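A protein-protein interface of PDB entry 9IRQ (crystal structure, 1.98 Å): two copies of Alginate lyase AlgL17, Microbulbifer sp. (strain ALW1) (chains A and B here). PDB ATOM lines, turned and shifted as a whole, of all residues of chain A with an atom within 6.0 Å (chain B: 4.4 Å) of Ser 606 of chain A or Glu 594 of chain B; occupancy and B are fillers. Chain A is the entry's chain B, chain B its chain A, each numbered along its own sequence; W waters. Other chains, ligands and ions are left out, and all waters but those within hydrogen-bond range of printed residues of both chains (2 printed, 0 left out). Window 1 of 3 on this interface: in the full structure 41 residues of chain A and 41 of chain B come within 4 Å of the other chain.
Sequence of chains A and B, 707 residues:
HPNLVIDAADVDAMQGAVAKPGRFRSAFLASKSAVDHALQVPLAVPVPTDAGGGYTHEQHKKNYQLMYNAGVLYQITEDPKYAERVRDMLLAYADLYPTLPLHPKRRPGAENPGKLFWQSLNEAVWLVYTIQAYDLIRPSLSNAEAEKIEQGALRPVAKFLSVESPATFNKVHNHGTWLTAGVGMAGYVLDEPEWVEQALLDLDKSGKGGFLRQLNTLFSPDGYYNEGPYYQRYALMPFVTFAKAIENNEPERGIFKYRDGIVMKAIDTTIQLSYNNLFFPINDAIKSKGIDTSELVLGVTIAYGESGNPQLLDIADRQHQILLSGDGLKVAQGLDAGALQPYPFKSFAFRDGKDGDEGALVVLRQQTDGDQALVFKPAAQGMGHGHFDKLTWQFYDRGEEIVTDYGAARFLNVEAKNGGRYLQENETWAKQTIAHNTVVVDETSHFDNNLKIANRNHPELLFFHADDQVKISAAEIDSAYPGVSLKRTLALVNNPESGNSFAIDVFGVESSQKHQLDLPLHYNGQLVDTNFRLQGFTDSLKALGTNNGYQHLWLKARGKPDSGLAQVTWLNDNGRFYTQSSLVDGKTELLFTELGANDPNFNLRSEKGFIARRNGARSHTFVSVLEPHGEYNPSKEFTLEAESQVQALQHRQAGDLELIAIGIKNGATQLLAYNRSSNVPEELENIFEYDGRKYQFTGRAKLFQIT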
ATOM      1  N   TRP A 554     -25.518  14.682 -17.177  1.00  0.00           N
ATOM      2  CA  TRP A 554     -26.261  13.925 -18.180  1.00  0.00           C
ATOM      3  C   TRP A 554     -25.286  13.036 -18.948  1.00  0.00           C
ATOM      4  O   TRP A 554     -24.194  13.473 -19.316  1.00  0.00           O
ATOM      5  CB  TRP A 554     -26.972  14.848 -19.181  1.00  0.00           C
ATOM      6  CG  TRP A 554     -27.931  15.893 -18.660  1.00  0.00           C
ATOM      7  CD1 TRP A 554     -27.808  17.252 -18.785  1.00  0.00           C
ATOM      8  CD2 TRP A 554     -29.181  15.665 -17.996  1.00  0.00           C
ATOM      9  NE1 TRP A 554     -28.894  17.883 -18.218  1.00  0.00           N
ATOM     10  CE2 TRP A 554     -29.752  16.929 -17.731  1.00  0.00           C
ATOM     11  CE3 TRP A 554     -29.865  14.516 -17.586  1.00  0.00           C
ATOM     12  CZ2 TRP A 554     -30.973  17.071 -17.079  1.00  0.00           C
ATOM     13  CZ3 TRP A 554     -31.074  14.659 -16.937  1.00  0.00           C
ATOM     14  CH2 TRP A 554     -31.618  15.928 -16.691  1.00  0.00           C
ATOM     15  N   LYS A 556     -24.568  11.788 -22.364  1.00  0.00           N
ATOM     16  CA  LYS A 556     -25.007  12.065 -23.726  1.00  0.00           C
ATOM     17  C   LYS A 556     -24.631  10.955 -24.699  1.00  0.00           C
ATOM     18  O   LYS A 556     -25.311  10.782 -25.717  1.00  0.00           O
ATOM     19  CB  LYS A 556     -24.446  13.407 -24.207  1.00  0.00           C
ATOM     20  CG  LYS A 556     -25.155  14.602 -23.532  1.00  0.00           C
ATOM     21  CD  LYS A 556     -24.934  15.908 -24.270  1.00  0.00           C
ATOM     22  CE  LYS A 556     -25.689  15.935 -25.591  1.00  0.00           C
ATOM     23  NZ  LYS A 556     -26.787  16.957 -25.620  1.00  0.00           N
ATOM     24  N   GLU A 594     -22.679  15.974 -20.293  1.00  0.00           N
ATOM     25  CA  GLU A 594     -22.992  17.391 -20.236  1.00  0.00           C
ATOM     26  C   GLU A 594     -23.513  17.661 -18.840  1.00  0.00           C
ATOM     27  O   GLU A 594     -24.352  16.912 -18.332  1.00  0.00           O
ATOM     28  CB  GLU A 594     -24.034  17.808 -21.281  1.00  0.00           C
ATOM     29  CG  GLU A 594     -24.405  19.287 -21.227  1.00  0.00           C
ATOM     30  CD  GLU A 594     -25.750  19.585 -21.877  1.00  0.00           C
ATOM     31  OE1 GLU A 594     -26.539  20.358 -21.273  1.00  0.00           O
ATOM     32  OE2 GLU A 594     -26.014  19.048 -22.984  1.00  0.00           O
ATOM     33  N   LEU A 595     -22.984  18.699 -18.213  1.00  0.00           N
ATOM     34  CA  LEU A 595     -23.415  19.071 -16.876  1.00  0.00           C
ATOM     35  C   LEU A 595     -24.811  19.683 -16.923  1.00  0.00           C
ATOM     36  O   LEU A 595     -25.131  20.455 -17.830  1.00  0.00           O
ATOM     37  CB  LEU A 595     -22.428  20.073 -16.296  1.00  0.00           C
ATOM     38  CG  LEU A 595     -22.630  20.448 -14.850  1.00  0.00           C
ATOM     39  CD1 LEU A 595     -22.467  19.181 -14.006  1.00  0.00           C
ATOM     40  CD2 LEU A 595     -21.574  21.477 -14.501  1.00  0.00           C
ATOM     41  N   GLY A 596     -25.652  19.344 -15.947  1.00  0.00           N
ATOM     42  CA  GLY A 596     -26.956  19.989 -15.926  1.00  0.00           C
ATOM     43  C   GLY A 596     -28.098  19.205 -15.311  1.00  0.00           C
ATOM     44  O   GLY A 596     -29.224  19.708 -15.232  1.00  0.00           O
ATOM     45  N   LEU A 604     -26.097  25.509 -12.821  1.00  0.00           N
ATOM     46  CA  LEU A 604     -24.871  24.952 -13.379  1.00  0.00           C
ATOM     47  C   LEU A 604     -24.725  25.299 -14.854  1.00  0.00           C
ATOM     48  O   LEU A 604     -25.715  25.460 -15.575  1.00  0.00           O
ATOM     49  CB  LEU A 604     -24.825  23.432 -13.196  1.00  0.00           C
ATOM     50  CG  LEU A 604     -24.863  22.966 -11.738  1.00  0.00           C
ATOM     51  CD1 LEU A 604     -25.097  21.467 -11.690  1.00  0.00           C
ATOM     52  CD2 LEU A 604     -23.581  23.325 -10.953  1.00  0.00           C
ATOM     53  N   ARG A 605     -23.476  25.427 -15.291  1.00  0.00           N
ATOM     54  CA  ARG A 605     -23.182  25.653 -16.702  1.00  0.00           C
ATOM     55  C   ARG A 605     -23.190  24.325 -17.450  1.00  0.00           C
ATOM     56  O   ARG A 605     -22.919  23.266 -16.876  1.00  0.00           O
ATOM     57  CB  ARG A 605     -21.821  26.338 -16.884  1.00  0.00           C
ATOM     58  CG  ARG A 605     -21.667  27.684 -16.167  1.00  0.00           C
ATOM     59  CD  ARG A 605     -20.357  28.353 -16.533  1.00  0.00           C
ATOM     60  NE  ARG A 605     -19.179  27.561 -16.151  1.00  0.00           N
ATOM     61  CZ  ARG A 605     -18.544  27.682 -14.985  1.00  0.00           C
ATOM     62  NH1 ARG A 605     -18.994  28.540 -14.086  1.00  0.00           N
ATOM     63  NH2 ARG A 605     -17.470  26.940 -14.705  1.00  0.00           N
ATOM     64  N   SER A 606     -23.528  24.386 -18.742  1.00  0.00           N
ATOM     65  CA  SER A 606     -23.628  23.193 -19.587  1.00  0.00           C
ATOM     66  C   SER A 606     -22.246  22.717 -20.050  1.00  0.00           C
ATOM     67  O   SER A 606     -21.973  22.568 -21.243  1.00  0.00           O
ATOM     68  CB  SER A 606     -24.527  23.484 -20.784  1.00  0.00           C
ATOM     69  OG  SER A 606     -25.797  23.926 -20.359  1.00  0.00           O
ATOM     70  N   GLU A 607     -21.372  22.454 -19.080  1.00  0.00           N
ATOM     71  CA  GLU A 607     -19.995  22.074 -19.383  1.00  0.00           C
ATOM     72  C   GLU A 607     -19.912  20.638 -19.907  1.00  0.00           C
ATOM     73  O   GLU A 607     -20.691  19.769 -19.513  1.00  0.00           O
ATOM     74  CB  GLU A 607     -19.114  22.217 -18.138  1.00  0.00           C
ATOM     75  CG  GLU A 607     -19.035  23.615 -17.553  1.00  0.00           C
ATOM     76  CD  GLU A 607     -18.111  24.556 -18.321  1.00  0.00           C
ATOM     77  OE1 GLU A 607     -18.277  25.789 -18.190  1.00  0.00           O
ATOM     78  OE2 GLU A 607     -17.213  24.082 -19.054  1.00  0.00           O
ATOM     79  N   LYS A 608     -18.943  20.388 -20.792  1.00  0.00           N
ATOM     80  CA  LYS A 608     -18.807  19.100 -21.465  1.00  0.00           C
ATOM     81  C   LYS A 608     -17.539  18.373 -21.022  1.00  0.00           C
ATOM     82  O   LYS A 608     -16.541  18.993 -20.640  1.00  0.00           O
ATOM     83  CB  LYS A 608     -18.767  19.271 -22.990  1.00  0.00           C
ATOM     84  CG  LYS A 608     -20.024  19.914 -23.585  1.00  0.00           C
ATOM     85  CD  LYS A 608     -19.833  20.188 -25.077  1.00  0.00           C
ATOM     86  CE  LYS A 608     -20.037  21.670 -25.423  1.00  0.00           C
ATOM     87  NZ  LYS A 608     -19.119  22.124 -26.512  1.00  0.00           N
ATOM     88  N   HIS B 552     -35.563  18.932 -31.651  1.00  0.00           N
ATOM     89  CA  HIS B 552     -34.192  19.225 -31.251  1.00  0.00           C
ATOM     90  C   HIS B 552     -34.097  19.982 -29.924  1.00  0.00           C
ATOM     91  O   HIS B 552     -32.995  20.106 -29.379  1.00  0.00           O
ATOM     92  CB  HIS B 552     -33.473  20.013 -32.364  1.00  0.00           C
ATOM     93  CG  HIS B 552     -33.281  19.242 -33.640  1.00  0.00           C
ATOM     94  ND1 HIS B 552     -32.656  18.011 -33.684  1.00  0.00           N
ATOM     95  CD2 HIS B 552     -33.602  19.542 -34.923  1.00  0.00           C
ATOM     96  CE1 HIS B 552     -32.607  17.587 -34.934  1.00  0.00           C
ATOM     97  NE2 HIS B 552     -33.169  18.500 -35.709  1.00  0.00           N
ATOM     98  N   LEU B 553     -35.215  20.437 -29.357  1.00  0.00           N
ATOM     99  CA  LEU B 553     -35.204  21.183 -28.093  1.00  0.00           C
ATOM    100  C   LEU B 553     -35.507  20.255 -26.923  1.00  0.00           C
ATOM    101  O   LEU B 553     -36.537  19.574 -26.922  1.00  0.00           O
ATOM    102  CB  LEU B 553     -36.227  22.324 -28.110  1.00  0.00           C
ATOM    103  CG  LEU B 553     -35.980  23.396 -29.168  1.00  0.00           C
ATOM    104  CD1 LEU B 553     -37.282  24.172 -29.518  1.00  0.00           C
ATOM    105  CD2 LEU B 553     -34.865  24.326 -28.702  1.00  0.00           C
ATOM    106  N   TRP B 554     -34.611  20.223 -25.935  1.00  0.00           N
ATOM    107  CA  TRP B 554     -34.953  19.657 -24.637  1.00  0.00           C
ATOM    108  C   TRP B 554     -35.855  20.644 -23.910  1.00  0.00           C
ATOM    109  O   TRP B 554     -35.589  21.852 -23.905  1.00  0.00           O
ATOM    110  CB  TRP B 554     -33.715  19.403 -23.760  1.00  0.00           C
ATOM    111  CG  TRP B 554     -32.646  18.499 -24.314  1.00  0.00           C
ATOM    112  CD1 TRP B 554     -31.342  18.828 -24.569  1.00  0.00           C
ATOM    113  CD2 TRP B 554     -32.775  17.112 -24.632  1.00  0.00           C
ATOM    114  NE1 TRP B 554     -30.667  17.742 -25.058  1.00  0.00           N
ATOM    115  CE2 TRP B 554     -31.524  16.676 -25.111  1.00  0.00           C
ATOM    116  CE3 TRP B 554     -33.840  16.208 -24.598  1.00  0.00           C
ATOM    117  CZ2 TRP B 554     -31.302  15.374 -25.536  1.00  0.00           C
ATOM    118  CZ3 TRP B 554     -33.617  14.916 -25.015  1.00  0.00           C
ATOM    119  CH2 TRP B 554     -32.358  14.509 -25.479  1.00  0.00           C
ATOM    120  N   LYS B 556     -36.465  21.953 -20.558  1.00  0.00           N
ATOM    121  CA  LYS B 556     -35.834  21.926 -19.244  1.00  0.00           C
ATOM    122  C   LYS B 556     -36.781  22.347 -18.122  1.00  0.00           C
ATOM    123  O   LYS B 556     -36.579  21.945 -16.971  1.00  0.00           O
ATOM    124  CB  LYS B 556     -34.605  22.834 -19.228  1.00  0.00           C
ATOM    125  CG  LYS B 556     -33.368  22.200 -19.865  1.00  0.00           C
ATOM    126  CD  LYS B 556     -32.113  22.936 -19.461  1.00  0.00           C
ATOM    127  CE  LYS B 556     -31.090  21.986 -18.902  1.00  0.00           C
ATOM    128  NZ  LYS B 556     -31.372  21.620 -17.475  1.00  0.00           N
ATOM    129  N   THR B 593     -36.091  26.012 -22.768  1.00  0.00           N
ATOM    130  CA  THR B 593     -35.544  24.975 -23.621  1.00  0.00           C
ATOM    131  C   THR B 593     -34.023  25.009 -23.612  1.00  0.00           C
ATOM    132  O   THR B 593     -33.402  26.022 -23.287  1.00  0.00           O
ATOM    133  CB  THR B 593     -36.031  25.119 -25.071  1.00  0.00           C
ATOM    134  OG1 THR B 593     -35.598  26.381 -25.608  1.00  0.00           O
ATOM    135  CG2 THR B 593     -37.540  25.034 -25.144  1.00  0.00           C
ATOM    136  N   GLU B 594     -33.431  23.882 -23.999  1.00  0.00           N
ATOM    137  CA  GLU B 594     -32.009  23.798 -24.317  1.00  0.00           C
ATOM    138  C   GLU B 594     -31.882  22.989 -25.596  1.00  0.00           C
ATOM    139  O   GLU B 594     -32.439  21.893 -25.685  1.00  0.00           O
ATOM    140  CB  GLU B 594     -31.185  23.143 -23.203  1.00  0.00           C
ATOM    141  CG  GLU B 594     -29.761  22.845 -23.665  1.00  0.00           C
ATOM    142  CD  GLU B 594     -28.900  22.166 -22.624  1.00  0.00           C
ATOM    143  OE1 GLU B 594     -27.925  21.502 -23.030  1.00  0.00           O
ATOM    144  OE2 GLU B 594     -29.176  22.297 -21.413  1.00  0.00           O
ATOM    145  N   LEU B 595     -31.205  23.515 -26.606  1.00  0.00           N
ATOM    146  CA  LEU B 595     -30.974  22.772 -27.874  1.00  0.00           C
ATOM    147  C   LEU B 595     -30.080  21.553 -27.627  1.00  0.00           C
ATOM    148  O   LEU B 595     -29.164  21.666 -26.820  1.00  0.00           O
ATOM    149  CB  LEU B 595     -30.360  23.704 -28.913  1.00  0.00           C
ATOM    150  CG  LEU B 595     -30.320  23.192 -30.346  1.00  0.00           C
ATOM    151  CD1 LEU B 595     -31.720  22.955 -30.868  1.00  0.00           C
ATOM    152  CD2 LEU B 595     -29.587  24.171 -31.234  1.00  0.00           C
ATOM    153  N   GLY B 596     -30.354  20.439 -28.311  1.00  0.00           N
ATOM    154  CA  GLY B 596     -29.500  19.248 -28.191  1.00  0.00           C
ATOM    155  C   GLY B 596     -30.186  17.905 -28.347  1.00  0.00           C
ATOM    156  O   GLY B 596     -29.506  16.905 -28.292  1.00  0.00           O
ATOM    157  N   SER B 606     -25.510  23.999 -27.372  1.00  0.00           N
ATOM    158  CA  SER B 606     -26.478  23.946 -26.279  1.00  0.00           C
ATOM    159  C   SER B 606     -27.160  25.289 -26.014  1.00  0.00           C
ATOM    160  O   SER B 606     -27.184  25.754 -24.872  1.00  0.00           O
ATOM    161  CB  SER B 606     -25.795  23.474 -24.988  1.00  0.00           C
ATOM    162  OG  SER B 606     -25.174  22.232 -25.202  1.00  0.00           O
ATOM    163  N   GLU B 607     -27.744  25.902 -27.036  1.00  0.00           N
ATOM    164  CA  GLU B 607     -28.342  27.215 -26.872  1.00  0.00           C
ATOM    165  C   GLU B 607     -29.613  27.166 -26.023  1.00  0.00           C
ATOM    166  O   GLU B 607     -30.329  26.163 -25.981  1.00  0.00           O
ATOM    167  CB  GLU B 607     -28.647  27.813 -28.244  1.00  0.00           C
ATOM    168  CG  GLU B 607     -27.416  27.920 -29.126  1.00  0.00           C
ATOM    169  CD  GLU B 607     -26.555  29.135 -28.800  1.00  0.00           C
ATOM    170  OE1 GLU B 607     -27.071  30.084 -28.159  1.00  0.00           O
ATOM    171  OE2 GLU B 607     -25.360  29.149 -29.185  1.00  0.00           O
HETATM  172  O   HOH W   1     -27.239  25.587 -21.980  1.00  0.00           O
HETATM  173  O   HOH W   2     -23.060  21.407 -23.994  1.00  0.00           O
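The side-chain carboxylate (OE1) of Glu 594 of chain B lies close to the side-chain carboxylate (OE1) of Glu 594 of chain A.
The side-chain amino group (NZ) of Lys 556 of chain A is in salt-bridge range of the side-chain carboxylate (OE2) of Glu 594 of chain A. O of Glu 594 of chain B is in hydrogen-bond range of N of Trp 554 of chain B (2.8 Å). The backbone NH (N) of Gly 596 of chain B sits at hydrogen-bond distance from the backbone carbonyl oxygen (O) of His 552 of chain B. The backbone NH (N) of Trp 554 of chain A sits at hydrogen-bond distance from the backbone carbonyl oxygen (O) of Glu 594 of chain A.
NE1 of Trp 554 of chain B touches NZ of Lys 556 of chain A, at 3.998 Å. Lys 556 of chain A touches Gly 596 of chain B (NZ to O, 3.8 Å). Ser 606 of chain B touches Glu 594 of chain A (OG to OE2, 3.97 Å). Lys 556 of chain B touches Gly 596 of chain A (NZ to O, 3.6 Å). Ser 606 of chain A touches Glu 594 of chain B (OG to OE2, 3.9 Å).
Of chain B, only Glu 594 (3.9 Å) comes within 4 Å of Ser 606 of chain A. Of the printed residues of chain A, Lys 556 of chain B touches Gly 596. Of the printed residues of chain B, Lys 556 of chain A touches Trp 554 and Gly 596. Of the printed residues of chain A, Gly 596 of chain B touches Lys 556 (3.8 Å). Printed residues of chain B within 4 Å of Gly 596 of chain A: Lys 556 (3.6 Å). The nearest printed residue of chain A that does not touch Lys 556 of chain B is Trp 554 of chain A (4.5 Å).
Printed residues of chain B that touch a printed residue of chain A: Trp 554, Lys 556, Glu 594, Gly 596 and Ser 606. Hydrophobic or aromatic side chains of chain B within 4 Å of the printed part of chain A: Trp 554. Printed residues of chain A that touch a printed residue of chain B: Lys 556, Glu 594, Gly 596 and Ser 606. Among the printed residues, no Asp or Glu carboxylate lies within 4 Å of a Lys or Arg side-chain nitrogen of the other chain.
Lys 556 of chain A touches Trp 554 of chain B, but with the chains exchanged Trp 554 of chain A does not touch Lys 556 of chain B (4.5 Å). Lys 556 of chain A touches Gly 596 of chain B, and with the chains exchanged Gly 596 of chain A touches Lys 556 of chain B. Glu 594 of chain B touches its own counterpart, Glu 594 of chain A. Glu 594 of chain A touches Ser 606 of chain B, and with the chains exchanged Ser 606 of chain A touches Glu 594 of chain B. Positions printed for both chains: 554, 556, 594, 595, 596, 606 and 607. Of the 6 pairs that touch across the chains among the printed residues, 5 have their exchanged pair printed and touching as well.
Water W2 bridges the side-chain hydroxyl of Ser 606 of chain B (2.6 Å) and the backbone carbonyl oxygen of Ser 606 of chain A (3.2 Å). Water W1 lies within hydrogen-bond range of OG of Ser 606 of chain A (2.7 Å) and O of Ser 606 of chain B (2.9 Å).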
